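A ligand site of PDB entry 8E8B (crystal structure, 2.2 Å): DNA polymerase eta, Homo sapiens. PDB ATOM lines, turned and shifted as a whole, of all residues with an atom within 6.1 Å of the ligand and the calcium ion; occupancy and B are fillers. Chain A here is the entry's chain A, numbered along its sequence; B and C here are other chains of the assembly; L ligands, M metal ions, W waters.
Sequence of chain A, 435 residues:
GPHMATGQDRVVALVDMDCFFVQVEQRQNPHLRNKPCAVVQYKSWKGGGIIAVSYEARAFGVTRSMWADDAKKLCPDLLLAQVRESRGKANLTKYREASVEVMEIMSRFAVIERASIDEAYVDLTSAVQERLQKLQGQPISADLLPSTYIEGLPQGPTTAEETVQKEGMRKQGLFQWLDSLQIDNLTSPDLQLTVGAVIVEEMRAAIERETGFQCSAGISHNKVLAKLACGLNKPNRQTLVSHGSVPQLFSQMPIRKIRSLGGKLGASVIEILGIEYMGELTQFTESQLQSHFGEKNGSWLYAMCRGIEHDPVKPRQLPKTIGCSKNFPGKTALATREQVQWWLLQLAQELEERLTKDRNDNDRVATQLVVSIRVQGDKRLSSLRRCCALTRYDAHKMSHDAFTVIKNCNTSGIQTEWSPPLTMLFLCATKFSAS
NE of Arg 58 sits at hydrogen-bond distance from O of Val 53 (2.9 Å). N3 of U 8 of chain C lies close to N1 of DA 5 of chain B, at 2.6 Å. The side-chain carboxylate of Asp 18 lies within salt-bridge range of the side-chain amino group of Lys 234 (2.8 Å). The backbone carbonyl oxygen (O) of Ile 51 sits at hydrogen-bond distance from the guanidinium group (NH2) of Arg 64 (3.0 Å). N of Asp 118 sits close to OG of Ser 116. The side-chain carboxylate of Asp 16 lies within salt-bridge range of the side-chain amino group of Lys 227, 3.7 Å away. The side-chain hydroxyl of Tyr 55 sits at hydrogen-bond distance from the guanidinium group of Arg 58 (3.1 Å). O3' of U 8 of chain C sits at hydrogen-bond distance from the side-chain hydroxyl (OG) of Ser 116.
The calcium ion is bound by an oxygen (O6) of the ligand, the side-chain carboxylate (OD2) of Asp 118, the side-chain carboxylate (OD1) of Asp 16, the backbone carbonyl oxygen (O) of Met 17, an oxygen (O2) of the ligand and an oxygen (O8) of the ligand.
A nitrogen (N4) of the ligand sits at hydrogen-bond distance from O4' of DA 5 of chain B. O2 of DT 4 of chain B is in hydrogen-bond range of N3 of the ligand, at 2.5 Å. The backbone NH (N) of Phe 20 sits at hydrogen-bond distance from an oxygen (O12) of the ligand, at 3.1 Å. The guanidinium group (NH2) of Arg 64 is in salt-bridge range of an oxygen (O5) of the ligand, at 3.4 Å. NH1 of Arg 58 lies within salt-bridge range of O3 of the ligand, at 3.0 Å. The side-chain amide oxygen of Gln 41 sits at hydrogen-bond distance from a nitrogen (N4) of the ligand. N of Phe 21 sits at hydrogen-bond distance from O12 of the ligand (3.1 Å). N of Cys 19 lies within hydrogen-bond range of O1 of the ligand, at 2.7 Å. An oxygen (O1) of the ligand sits at hydrogen-bond distance from the side-chain hydroxyl (OH) of Tyr 55. A nitrogen (N3) of the ligand is in hydrogen-bond range of N3 of DA 5 of chain B (3.4 Å). NZ of Lys 234 is in salt-bridge range of O1 of the ligand, 3.3 Å away.
O10 of the ligand sits close to O2' of U 8 of chain C, 3.2 Å away. Asp 18 touches the ligand (CA to O1, 3.2 Å). O of Ile 51 touches C4 of the ligand, at 3.5 Å. Ala 52 touches the ligand. Ile 117 touches the ligand. Hydrophobic or aromatic side chains within 4 Å of the ligand: Phe 20, Phe 21, Ile 51, Ala 52, Tyr 55 and Ile 117. 18 residues have an atom within 4 Å of the ligand: Asp 16, Met 17, Asp 18, Cys 19, Phe 20, Phe 21, Gln 41, Ile 51, Ala 52, Tyr 55, Arg 58, Arg 64, Ile 117, Asp 118, Lys 234, DT 4 of chain B, DA 5 of chain B and U 8 of chain C. Along chain A the residues within 4 Å of the ligand span positions 16 to 234.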
ATOM      1  N   ASP A  16      27.487 -13.272 -27.621  1.00  0.00           N
ATOM      2  CA  ASP A  16      27.145 -14.324 -26.661  1.00  0.00           C
ATOM      3  C   ASP A  16      25.893 -15.030 -27.151  1.00  0.00           C
ATOM      4  O   ASP A  16      24.824 -14.414 -27.210  1.00  0.00           O
ATOM      5  CB  ASP A  16      26.902 -13.701 -25.295  1.00  0.00           C
ATOM      6  CG  ASP A  16      26.860 -14.715 -24.225  1.00  0.00           C
ATOM      7  OD1 ASP A  16      25.964 -15.582 -24.297  1.00  0.00           O
ATOM      8  OD2 ASP A  16      27.675 -14.627 -23.281  1.00  0.00           O
ATOM      9  N   MET A  17      26.009 -16.317 -27.470  1.00  0.00           N
ATOM     10  CA  MET A  17      24.845 -17.088 -27.879  1.00  0.00           C
ATOM     11  C   MET A  17      23.883 -17.258 -26.714  1.00  0.00           C
ATOM     12  O   MET A  17      24.266 -17.731 -25.655  1.00  0.00           O
ATOM     13  CB  MET A  17      25.249 -18.453 -28.454  1.00  0.00           C
ATOM     14  CG  MET A  17      26.511 -18.468 -29.311  1.00  0.00           C
ATOM     15  SD  MET A  17      26.222 -17.296 -30.662  1.00  0.00           S
ATOM     16  CE  MET A  17      24.710 -17.975 -31.347  1.00  0.00           C
ATOM     17  N   ASP A  18      22.642 -16.858 -26.912  1.00  0.00           N
ATOM     18  CA  ASP A  18      21.617 -17.021 -25.881  1.00  0.00           C
ATOM     19  C   ASP A  18      21.406 -18.499 -25.555  1.00  0.00           C
ATOM     20  O   ASP A  18      21.230 -19.328 -26.457  1.00  0.00           O
ATOM     21  CB  ASP A  18      20.299 -16.400 -26.366  1.00  0.00           C
ATOM     22  CG  ASP A  18      20.433 -14.932 -26.717  1.00  0.00           C
ATOM     23  OD1 ASP A  18      21.271 -14.252 -26.121  1.00  0.00           O
ATOM     24  OD2 ASP A  18      19.693 -14.464 -27.574  1.00  0.00           O
ATOM     25  N   CYS A  19      21.411 -18.826 -24.248  1.00  0.00           N
ATOM     26  CA  CYS A  19      21.230 -20.183 -23.735  1.00  0.00           C
ATOM     27  C   CYS A  19      21.673 -21.236 -24.736  1.00  0.00           C
ATOM     28  O   CYS A  19      20.852 -21.970 -25.277  1.00  0.00           O
ATOM     29  CB  CYS A  19      19.755 -20.429 -23.319  1.00  0.00           C
ATOM     30  SG  CYS A  19      18.508 -20.006 -24.584  1.00  0.00           S
ATOM     31  N   PHE A  20      22.981 -21.313 -24.979  1.00  0.00           N
ATOM     32  CA  PHE A  20      23.486 -21.927 -26.199  1.00  0.00           C
ATOM     33  C   PHE A  20      23.136 -23.411 -26.292  1.00  0.00           C
ATOM     34  O   PHE A  20      22.660 -23.883 -27.344  1.00  0.00           O
ATOM     35  CB  PHE A  20      24.990 -21.724 -26.285  1.00  0.00           C
ATOM     36  CG  PHE A  20      25.567 -22.261 -27.538  1.00  0.00           C
ATOM     37  CD1 PHE A  20      24.980 -21.950 -28.748  1.00  0.00           C
ATOM     38  CD2 PHE A  20      26.670 -23.098 -27.516  1.00  0.00           C
ATOM     39  CE1 PHE A  20      25.498 -22.444 -29.938  1.00  0.00           C
ATOM     40  CE2 PHE A  20      27.196 -23.598 -28.696  1.00  0.00           C
ATOM     41  CZ  PHE A  20      26.598 -23.267 -29.906  1.00  0.00           C
ATOM     42  N   PHE A  21      23.408 -24.176 -25.246  1.00  0.00           N
ATOM     43  CA  PHE A  21      23.128 -25.612 -25.328  1.00  0.00           C
ATOM     44  C   PHE A  21      21.643 -25.867 -25.596  1.00  0.00           C
ATOM     45  O   PHE A  21      21.294 -26.752 -26.383  1.00  0.00           O
ATOM     46  CB  PHE A  21      23.589 -26.341 -24.053  1.00  0.00           C
ATOM     47  CG  PHE A  21      25.079 -26.486 -23.894  1.00  0.00           C
ATOM     48  CD1 PHE A  21      25.966 -25.632 -24.519  1.00  0.00           C
ATOM     49  CD2 PHE A  21      25.599 -27.540 -23.135  1.00  0.00           C
ATOM     50  CE1 PHE A  21      27.375 -25.801 -24.359  1.00  0.00           C
ATOM     51  CE2 PHE A  21      26.979 -27.714 -22.976  1.00  0.00           C
ATOM     52  CZ  PHE A  21      27.862 -26.837 -23.594  1.00  0.00           C
ATOM     53  N   VAL A  22      20.768 -25.069 -24.967  1.00  0.00           N
ATOM     54  CA  VAL A  22      19.334 -25.179 -25.211  1.00  0.00           C
ATOM     55  C   VAL A  22      18.999 -24.910 -26.676  1.00  0.00           C
ATOM     56  O   VAL A  22      18.220 -25.630 -27.293  1.00  0.00           O
ATOM     57  CB  VAL A  22      18.560 -24.231 -24.286  1.00  0.00           C
ATOM     58  CG1 VAL A  22      17.096 -24.192 -24.707  1.00  0.00           C
ATOM     59  CG2 VAL A  22      18.708 -24.685 -22.859  1.00  0.00           C
ATOM     60  N   GLN A  41      22.730 -32.609 -17.370  1.00  0.00           N
ATOM     61  CA  GLN A  41      23.784 -33.636 -17.410  1.00  0.00           C
ATOM     62  C   GLN A  41      23.430 -34.710 -16.385  1.00  0.00           C
ATOM     63  O   GLN A  41      23.181 -34.380 -15.215  1.00  0.00           O
ATOM     64  CB  GLN A  41      25.173 -33.067 -17.080  1.00  0.00           C
ATOM     65  CG  GLN A  41      25.760 -32.089 -18.070  1.00  0.00           C
ATOM     66  CD  GLN A  41      27.194 -31.643 -17.749  1.00  0.00           C
ATOM     67  OE1 GLN A  41      28.051 -31.641 -18.630  1.00  0.00           O
ATOM     68  NE2 GLN A  41      27.452 -31.227 -16.497  1.00  0.00           N
ATOM     69  N   ILE A  51      22.244 -27.167 -16.757  1.00  0.00           N
ATOM     70  CA  ILE A  51      23.354 -26.310 -17.141  1.00  0.00           C
ATOM     71  C   ILE A  51      22.971 -25.220 -18.145  1.00  0.00           C
ATOM     72  O   ILE A  51      23.812 -24.359 -18.442  1.00  0.00           O
ATOM     73  CB  ILE A  51      24.547 -27.123 -17.693  1.00  0.00           C
ATOM     74  CG1 ILE A  51      24.109 -28.063 -18.821  1.00  0.00           C
ATOM     75  CG2 ILE A  51      25.236 -27.898 -16.548  1.00  0.00           C
ATOM     76  CD1 ILE A  51      25.262 -28.758 -19.511  1.00  0.00           C
ATOM     77  N   ALA A  52      21.748 -25.220 -18.682  1.00  0.00           N
ATOM     78  CA  ALA A  52      21.335 -24.177 -19.622  1.00  0.00           C
ATOM     79  C   ALA A  52      19.806 -24.116 -19.631  1.00  0.00           C
ATOM     80  O   ALA A  52      19.139 -25.149 -19.555  1.00  0.00           O
ATOM     81  CB  ALA A  52      21.856 -24.421 -21.057  1.00  0.00           C
ATOM     82  N   VAL A  53      19.269 -22.905 -19.696  1.00  0.00           N
ATOM     83  CA  VAL A  53      17.854 -22.677 -19.458  1.00  0.00           C
ATOM     84  C   VAL A  53      17.375 -21.690 -20.497  1.00  0.00           C
ATOM     85  O   VAL A  53      17.941 -20.605 -20.621  1.00  0.00           O
ATOM     86  CB  VAL A  53      17.593 -22.125 -18.041  1.00  0.00           C
ATOM     87  CG1 VAL A  53      16.109 -22.197 -17.705  1.00  0.00           C
ATOM     88  CG2 VAL A  53      18.407 -22.861 -17.032  1.00  0.00           C
ATOM     89  N   TYR A  55      14.784 -18.849 -22.048  1.00  0.00           N
ATOM     90  CA  TYR A  55      14.282 -17.667 -21.363  1.00  0.00           C
ATOM     91  C   TYR A  55      12.840 -17.870 -20.899  1.00  0.00           C
ATOM     92  O   TYR A  55      12.473 -17.394 -19.809  1.00  0.00           O
ATOM     93  CB  TYR A  55      14.440 -16.446 -22.266  1.00  0.00           C
ATOM     94  CG  TYR A  55      15.877 -15.976 -22.221  1.00  0.00           C
ATOM     95  CD1 TYR A  55      16.881 -16.682 -22.898  1.00  0.00           C
ATOM     96  CD2 TYR A  55      16.251 -14.873 -21.465  1.00  0.00           C
ATOM     97  CE1 TYR A  55      18.213 -16.269 -22.844  1.00  0.00           C
ATOM     98  CE2 TYR A  55      17.587 -14.437 -21.409  1.00  0.00           C
ATOM     99  CZ  TYR A  55      18.561 -15.139 -22.091  1.00  0.00           C
ATOM    100  OH  TYR A  55      19.892 -14.722 -22.022  1.00  0.00           O
ATOM    101  N   ARG A  58      13.389 -19.657 -17.708  1.00  0.00           N
ATOM    102  CA  ARG A  58      13.893 -18.705 -16.705  1.00  0.00           C
ATOM    103  C   ARG A  58      12.777 -17.851 -16.100  1.00  0.00           C
ATOM    104  O   ARG A  58      12.874 -17.446 -14.926  1.00  0.00           O
ATOM    105  CB  ARG A  58      14.946 -17.775 -17.319  1.00  0.00           C
ATOM    106  CG  ARG A  58      16.245 -18.444 -17.722  1.00  0.00           C
ATOM    107  CD  ARG A  58      17.208 -17.421 -18.329  1.00  0.00           C
ATOM    108  NE  ARG A  58      18.238 -18.101 -19.102  1.00  0.00           N
ATOM    109  CZ  ARG A  58      19.350 -17.518 -19.538  1.00  0.00           C
ATOM    110  NH1 ARG A  58      19.582 -16.222 -19.371  1.00  0.00           N
ATOM    111  NH2 ARG A  58      20.252 -18.261 -20.175  1.00  0.00           N
ATOM    112  N   ARG A  64      20.541 -22.237 -13.860  1.00  0.00           N
ATOM    113  CA  ARG A  64      21.637 -23.214 -13.965  1.00  0.00           C
ATOM    114  C   ARG A  64      22.129 -23.656 -12.587  1.00  0.00           C
ATOM    115  O   ARG A  64      21.893 -23.041 -11.471  1.00  0.00           O
ATOM    116  CB  ARG A  64      22.800 -22.620 -14.773  1.00  0.00           C
ATOM    117  CG  ARG A  64      24.065 -22.379 -13.960  1.00  0.00           C
ATOM    118  CD  ARG A  64      25.270 -22.043 -14.823  1.00  0.00           C
ATOM    119  NE  ARG A  64      24.991 -22.208 -16.241  1.00  0.00           N
ATOM    120  CZ  ARG A  64      24.716 -21.222 -17.075  1.00  0.00           C
ATOM    121  NH1 ARG A  64      24.677 -19.976 -16.632  1.00  0.00           N
ATOM    122  NH2 ARG A  64      24.472 -21.472 -18.350  1.00  0.00           N
ATOM    123  N   LEU A  92      30.597 -33.368 -24.669  1.00  0.00           N
ATOM    124  CA  LEU A  92      30.036 -32.095 -25.107  1.00  0.00           C
ATOM    125  C   LEU A  92      30.310 -31.816 -26.575  1.00  0.00           C
ATOM    126  O   LEU A  92      30.294 -30.656 -26.997  1.00  0.00           O
ATOM    127  CB  LEU A  92      30.542 -30.946 -24.220  1.00  0.00           C
ATOM    128  CG  LEU A  92      30.352 -31.101 -22.717  1.00  0.00           C
ATOM    129  CD1 LEU A  92      30.989 -29.945 -21.970  1.00  0.00           C
ATOM    130  CD2 LEU A  92      28.887 -31.203 -22.384  1.00  0.00           C
ATOM    131  N   SER A 116      34.817 -18.287 -24.737  1.00  0.00           N
ATOM    132  CA  SER A 116      34.351 -19.576 -24.225  1.00  0.00           C
ATOM    133  C   SER A 116      33.567 -20.237 -25.361  1.00  0.00           C
ATOM    134  O   SER A 116      33.362 -19.635 -26.416  1.00  0.00           O
ATOM    135  CB  SER A 116      33.468 -19.407 -22.984  1.00  0.00           C
ATOM    136  OG  SER A 116      32.139 -19.130 -23.373  1.00  0.00           O
ATOM    137  N   ILE A 117      33.049 -21.445 -25.089  1.00  0.00           N
ATOM    138  CA  ILE A 117      32.372 -22.233 -26.115  1.00  0.00           C
ATOM    139  C   ILE A 117      31.296 -21.445 -26.835  1.00  0.00           C
ATOM    140  O   ILE A 117      30.973 -21.714 -27.998  1.00  0.00           O
ATOM    141  CB  ILE A 117      31.767 -23.518 -25.520  1.00  0.00           C
ATOM    142  CG1 ILE A 117      31.340 -24.483 -26.631  1.00  0.00           C
ATOM    143  CG2 ILE A 117      30.584 -23.194 -24.644  1.00  0.00           C
ATOM    144  CD1 ILE A 117      31.134 -25.890 -26.126  1.00  0.00           C
ATOM    145  N   ASP A 118      30.688 -20.460 -26.169  1.00  0.00           N
ATOM    146  CA  ASP A 118      29.599 -19.767 -26.845  1.00  0.00           C
ATOM    147  C   ASP A 118      29.734 -18.247 -26.758  1.00  0.00           C
ATOM    148  O   ASP A 118      28.731 -17.542 -26.938  1.00  0.00           O
ATOM    149  CB  ASP A 118      28.256 -20.202 -26.297  1.00  0.00           C
ATOM    150  CG  ASP A 118      27.913 -19.495 -25.041  1.00  0.00           C
ATOM    151  OD1 ASP A 118      28.822 -19.318 -24.200  1.00  0.00           O
ATOM    152  OD2 ASP A 118      26.730 -19.107 -24.895  1.00  0.00           O
ATOM    153  N   GLU A 119      30.935 -17.740 -26.484  1.00  0.00           N
ATOM    154  CA  GLU A 119      31.097 -16.296 -26.602  1.00  0.00           C
ATOM    155  C   GLU A 119      32.475 -15.939 -27.114  1.00  0.00           C
ATOM    156  O   GLU A 119      33.471 -16.618 -26.824  1.00  0.00           O
ATOM    157  CB  GLU A 119      30.785 -15.572 -25.282  1.00  0.00           C
ATOM    158  CG  GLU A 119      31.911 -15.415 -24.327  1.00  0.00           C
ATOM    159  CD  GLU A 119      31.402 -14.912 -22.989  1.00  0.00           C
ATOM    160  OE1 GLU A 119      30.335 -15.353 -22.535  1.00  0.00           O
ATOM    161  OE2 GLU A 119      32.120 -14.093 -22.365  1.00  0.00           O
ATOM    162  N   LYS A 227      31.395  -6.704 -22.798  1.00  0.00           N
ATOM    163  CA  LYS A 227      30.806  -7.828 -22.052  1.00  0.00           C
ATOM    164  C   LYS A 227      29.696  -7.357 -21.129  1.00  0.00           C
ATOM    165  O   LYS A 227      28.599  -7.927 -21.105  1.00  0.00           O
ATOM    166  CB  LYS A 227      31.921  -8.559 -21.280  1.00  0.00           C
ATOM    167  CG  LYS A 227      31.487  -9.662 -20.297  1.00  0.00           C
ATOM    168  CD  LYS A 227      30.875 -10.846 -21.010  1.00  0.00           C
ATOM    169  CE  LYS A 227      30.627 -12.014 -20.064  1.00  0.00           C
ATOM    170  NZ  LYS A 227      29.904 -13.100 -20.781  1.00  0.00           N
ATOM    171  N   LYS A 234      18.986  -8.811 -22.999  1.00  0.00           N
ATOM    172  CA  LYS A 234      18.949 -10.175 -23.530  1.00  0.00           C
ATOM    173  C   LYS A 234      17.505 -10.667 -23.412  1.00  0.00           C
ATOM    174  O   LYS A 234      16.750 -10.208 -22.551  1.00  0.00           O
ATOM    175  CB  LYS A 234      19.961 -11.014 -22.739  1.00  0.00           C
ATOM    176  CG  LYS A 234      21.423 -10.892 -23.138  1.00  0.00           C
ATOM    177  CD  LYS A 234      22.259 -12.060 -22.659  1.00  0.00           C
ATOM    178  CE  LYS A 234      23.293 -12.537 -23.654  1.00  0.00           C
ATOM    179  NZ  LYS A 234      23.098 -13.958 -24.053  1.00  0.00           N
ATOM    180  N   PRO A 235      17.090 -11.612 -24.282  1.00  0.00           N
ATOM    181  CA  PRO A 235      17.825 -12.248 -25.371  1.00  0.00           C
ATOM    182  C   PRO A 235      17.646 -11.557 -26.714  1.00  0.00           C
ATOM    183  O   PRO A 235      16.808 -10.659 -26.852  1.00  0.00           O
ATOM    184  CB  PRO A 235      17.229 -13.655 -25.392  1.00  0.00           C
ATOM    185  CG  PRO A 235      15.762 -13.385 -25.098  1.00  0.00           C
ATOM    186  CD  PRO A 235      15.747 -12.187 -24.144  1.00  0.00           C
ATOM    187  P    DT B   4      28.385 -31.712  -8.550  1.00  0.00           P
ATOM    188  OP1  DT B   4      28.340 -33.161  -8.129  1.00  0.00           O
ATOM    189  OP2  DT B   4      29.486 -30.906  -7.911  1.00  0.00           O
ATOM    190  O5'  DT B   4      28.629 -31.679 -10.128  1.00  0.00           O
ATOM    191  C5'  DT B   4      27.834 -32.554 -10.972  1.00  0.00           C
ATOM    192  C4'  DT B   4      28.284 -32.413 -12.403  1.00  0.00           C
ATOM    193  O4'  DT B   4      28.178 -31.042 -12.818  1.00  0.00           O
ATOM    194  C3'  DT B   4      29.724 -32.816 -12.664  1.00  0.00           C
ATOM    195  O3'  DT B   4      29.844 -33.319 -13.989  1.00  0.00           O
ATOM    196  C2'  DT B   4      30.456 -31.488 -12.598  1.00  0.00           C
ATOM    197  C1'  DT B   4      29.447 -30.567 -13.244  1.00  0.00           C
ATOM    198  N1   DT B   4      29.553 -29.175 -12.820  1.00  0.00           N
ATOM    199  C2   DT B   4      29.377 -28.200 -13.770  1.00  0.00           C
ATOM    200  O2   DT B   4      29.130 -28.457 -14.938  1.00  0.00           O
ATOM    201  N3   DT B   4      29.487 -26.913 -13.312  1.00  0.00           N
ATOM    202  C4   DT B   4      29.757 -26.531 -12.010  1.00  0.00           C
ATOM    203  O4   DT B   4      29.831 -25.334 -11.735  1.00  0.00           O
ATOM    204  C5   DT B   4      29.937 -27.601 -11.059  1.00  0.00           C
ATOM    205  C7   DT B   4      30.241 -27.269  -9.635  1.00  0.00           C
ATOM    206  C6   DT B   4      29.836 -28.863 -11.510  1.00  0.00           C
ATOM    207  P    DA B   5      31.206 -33.920 -14.543  1.00  0.00           P
ATOM    208  OP1  DA B   5      30.847 -35.195 -15.213  1.00  0.00           O
ATOM    209  OP2  DA B   5      32.259 -33.891 -13.486  1.00  0.00           O
ATOM    210  O5'  DA B   5      31.581 -32.905 -15.690  1.00  0.00           O
ATOM    211  C5'  DA B   5      30.734 -32.799 -16.803  1.00  0.00           C
ATOM    212  C4'  DA B   5      31.303 -31.842 -17.810  1.00  0.00           C
ATOM    213  O4'  DA B   5      31.226 -30.480 -17.288  1.00  0.00           O
ATOM    214  C3'  DA B   5      32.772 -32.080 -18.137  1.00  0.00           C
ATOM    215  O3'  DA B   5      32.957 -31.836 -19.505  1.00  0.00           O
ATOM    216  C2'  DA B   5      33.486 -31.040 -17.271  1.00  0.00           C
ATOM    217  C1'  DA B   5      32.505 -29.885 -17.334  1.00  0.00           C
ATOM    218  N9   DA B   5      32.580 -28.961 -16.224  1.00  0.00           N
ATOM    219  C8   DA B   5      32.773 -29.261 -14.903  1.00  0.00           C
ATOM    220  N7   DA B   5      32.753 -28.207 -14.120  1.00  0.00           N
ATOM    221  C5   DA B   5      32.530 -27.147 -14.981  1.00  0.00           C
ATOM    222  C6   DA B   5      32.413 -25.763 -14.783  1.00  0.00           C
ATOM    223  N6   DA B   5      32.505 -25.182 -13.591  1.00  0.00           N
ATOM    224  N1   DA B   5      32.191 -24.991 -15.865  1.00  0.00           N
ATOM    225  C2   DA B   5      32.084 -25.569 -17.074  1.00  0.00           C
ATOM    226  N3   DA B   5      32.193 -26.854 -17.387  1.00  0.00           N
ATOM    227  C4   DA B   5      32.409 -27.599 -16.285  1.00  0.00           C
ATOM    228  P     U C   8      30.190 -15.393 -16.353  1.00  0.00           P
ATOM    229  OP1   U C   8      29.508 -14.125 -16.837  1.00  0.00           O
ATOM    230  OP2   U C   8      29.649 -15.920 -15.036  1.00  0.00           O
ATOM    231  O5'   U C   8      29.958 -16.511 -17.480  1.00  0.00           O
ATOM    232  C5'   U C   8      30.786 -16.466 -18.662  1.00  0.00           C
ATOM    233  C4'   U C   8      31.107 -17.873 -19.096  1.00  0.00           C
ATOM    234  O4'   U C   8      31.652 -18.610 -17.983  1.00  0.00           O
ATOM    235  C3'   U C   8      29.920 -18.703 -19.571  1.00  0.00           C
ATOM    236  O3'   U C   8      29.958 -18.831 -20.980  1.00  0.00           O
ATOM    237  C2'   U C   8      30.136 -20.111 -19.007  1.00  0.00           C
ATOM    238  O2'   U C   8      30.284 -20.994 -20.110  1.00  0.00           O
ATOM    239  C1'   U C   8      31.421 -19.982 -18.185  1.00  0.00           C
ATOM    240  N1    U C   8      31.339 -20.618 -16.861  1.00  0.00           N
ATOM    241  C2    U C   8      31.736 -21.928 -16.761  1.00  0.00           C
ATOM    242  O2    U C   8      32.140 -22.579 -17.724  1.00  0.00           O
ATOM    243  N3    U C   8      31.657 -22.459 -15.507  1.00  0.00           N
ATOM    244  C4    U C   8      31.230 -21.823 -14.355  1.00  0.00           C
ATOM    245  O4    U C   8      31.211 -22.452 -13.296  1.00  0.00           O
ATOM    246  C5    U C   8      30.832 -20.457 -14.540  1.00  0.00           C
ATOM    247  C6    U C   8      30.900 -19.916 -15.761  1.00  0.00           C
HETATM  248  P1  LIG L   1      22.764 -16.819 -21.613  1.00  0.00           P
HETATM  249  O1  LIG L   1      21.733 -16.651 -22.732  1.00  0.00           O
HETATM  250  O2  LIG L   1      24.134 -16.450 -22.181  1.00  0.00           O
HETATM  251  O3  LIG L   1      22.407 -16.037 -20.352  1.00  0.00           O
HETATM  252  O4  LIG L   1      22.848 -18.404 -21.376  1.00  0.00           O
HETATM  253  P2  LIG L   1      23.914 -19.534 -21.724  1.00  0.00           P
HETATM  254  O5  LIG L   1      23.284 -20.906 -21.498  1.00  0.00           O
HETATM  255  O6  LIG L   1      24.522 -19.404 -23.079  1.00  0.00           O
HETATM  256  O7  LIG L   1      24.963 -19.345 -20.540  1.00  0.00           O
HETATM  257  P3  LIG L   1      26.536 -19.094 -20.553  1.00  0.00           P
HETATM  258  O8  LIG L   1      26.815 -18.213 -21.762  1.00  0.00           O
HETATM  259  O9  LIG L   1      26.955 -18.426 -19.272  1.00  0.00           O
HETATM  260  O10 LIG L   1      27.205 -20.530 -20.904  1.00  0.00           O
HETATM  261  C1  LIG L   1      27.273 -21.020 -22.261  1.00  0.00           C
HETATM  262  C2  LIG L   1      26.897 -22.473 -22.375  1.00  0.00           C
HETATM  263  O11 LIG L   1      27.906 -23.277 -21.730  1.00  0.00           O
HETATM  264  C3  LIG L   1      25.563 -22.858 -21.745  1.00  0.00           C
HETATM  265  O12 LIG L   1      24.501 -22.853 -22.695  1.00  0.00           O
HETATM  266  C4  LIG L   1      25.804 -24.303 -21.302  1.00  0.00           C
HETATM  267  C5  LIG L   1      27.304 -24.366 -21.034  1.00  0.00           C
HETATM  268  N1  LIG L   1      27.656 -24.248 -19.603  1.00  0.00           N
HETATM  269  C6  LIG L   1      27.582 -23.148 -18.779  1.00  0.00           C
HETATM  270  N2  LIG L   1      27.976 -23.428 -17.536  1.00  0.00           N
HETATM  271  C7  LIG L   1      28.304 -24.774 -17.572  1.00  0.00           C
HETATM  272  C8  LIG L   1      28.699 -25.690 -16.564  1.00  0.00           C
HETATM  273  O13 LIG L   1      28.864 -25.350 -15.392  1.00  0.00           O
HETATM  274  N3  LIG L   1      28.867 -26.989 -16.882  1.00  0.00           N
HETATM  275  C9  LIG L   1      28.658 -27.346 -18.209  1.00  0.00           C
HETATM  276  N4  LIG L   1      28.791 -28.655 -18.475  1.00  0.00           N
HETATM  277  N5  LIG L   1      28.297 -26.535 -19.196  1.00  0.00           N
HETATM  278  C10 LIG L   1      28.127 -25.273 -18.828  1.00  0.00           C
HETATM  279 CA    CA M   1      25.440 -17.701 -23.678  1.00  0.00          CA
HETATM  280  O   HOH W   1      28.572 -16.126 -20.587  1.00  0.00           O
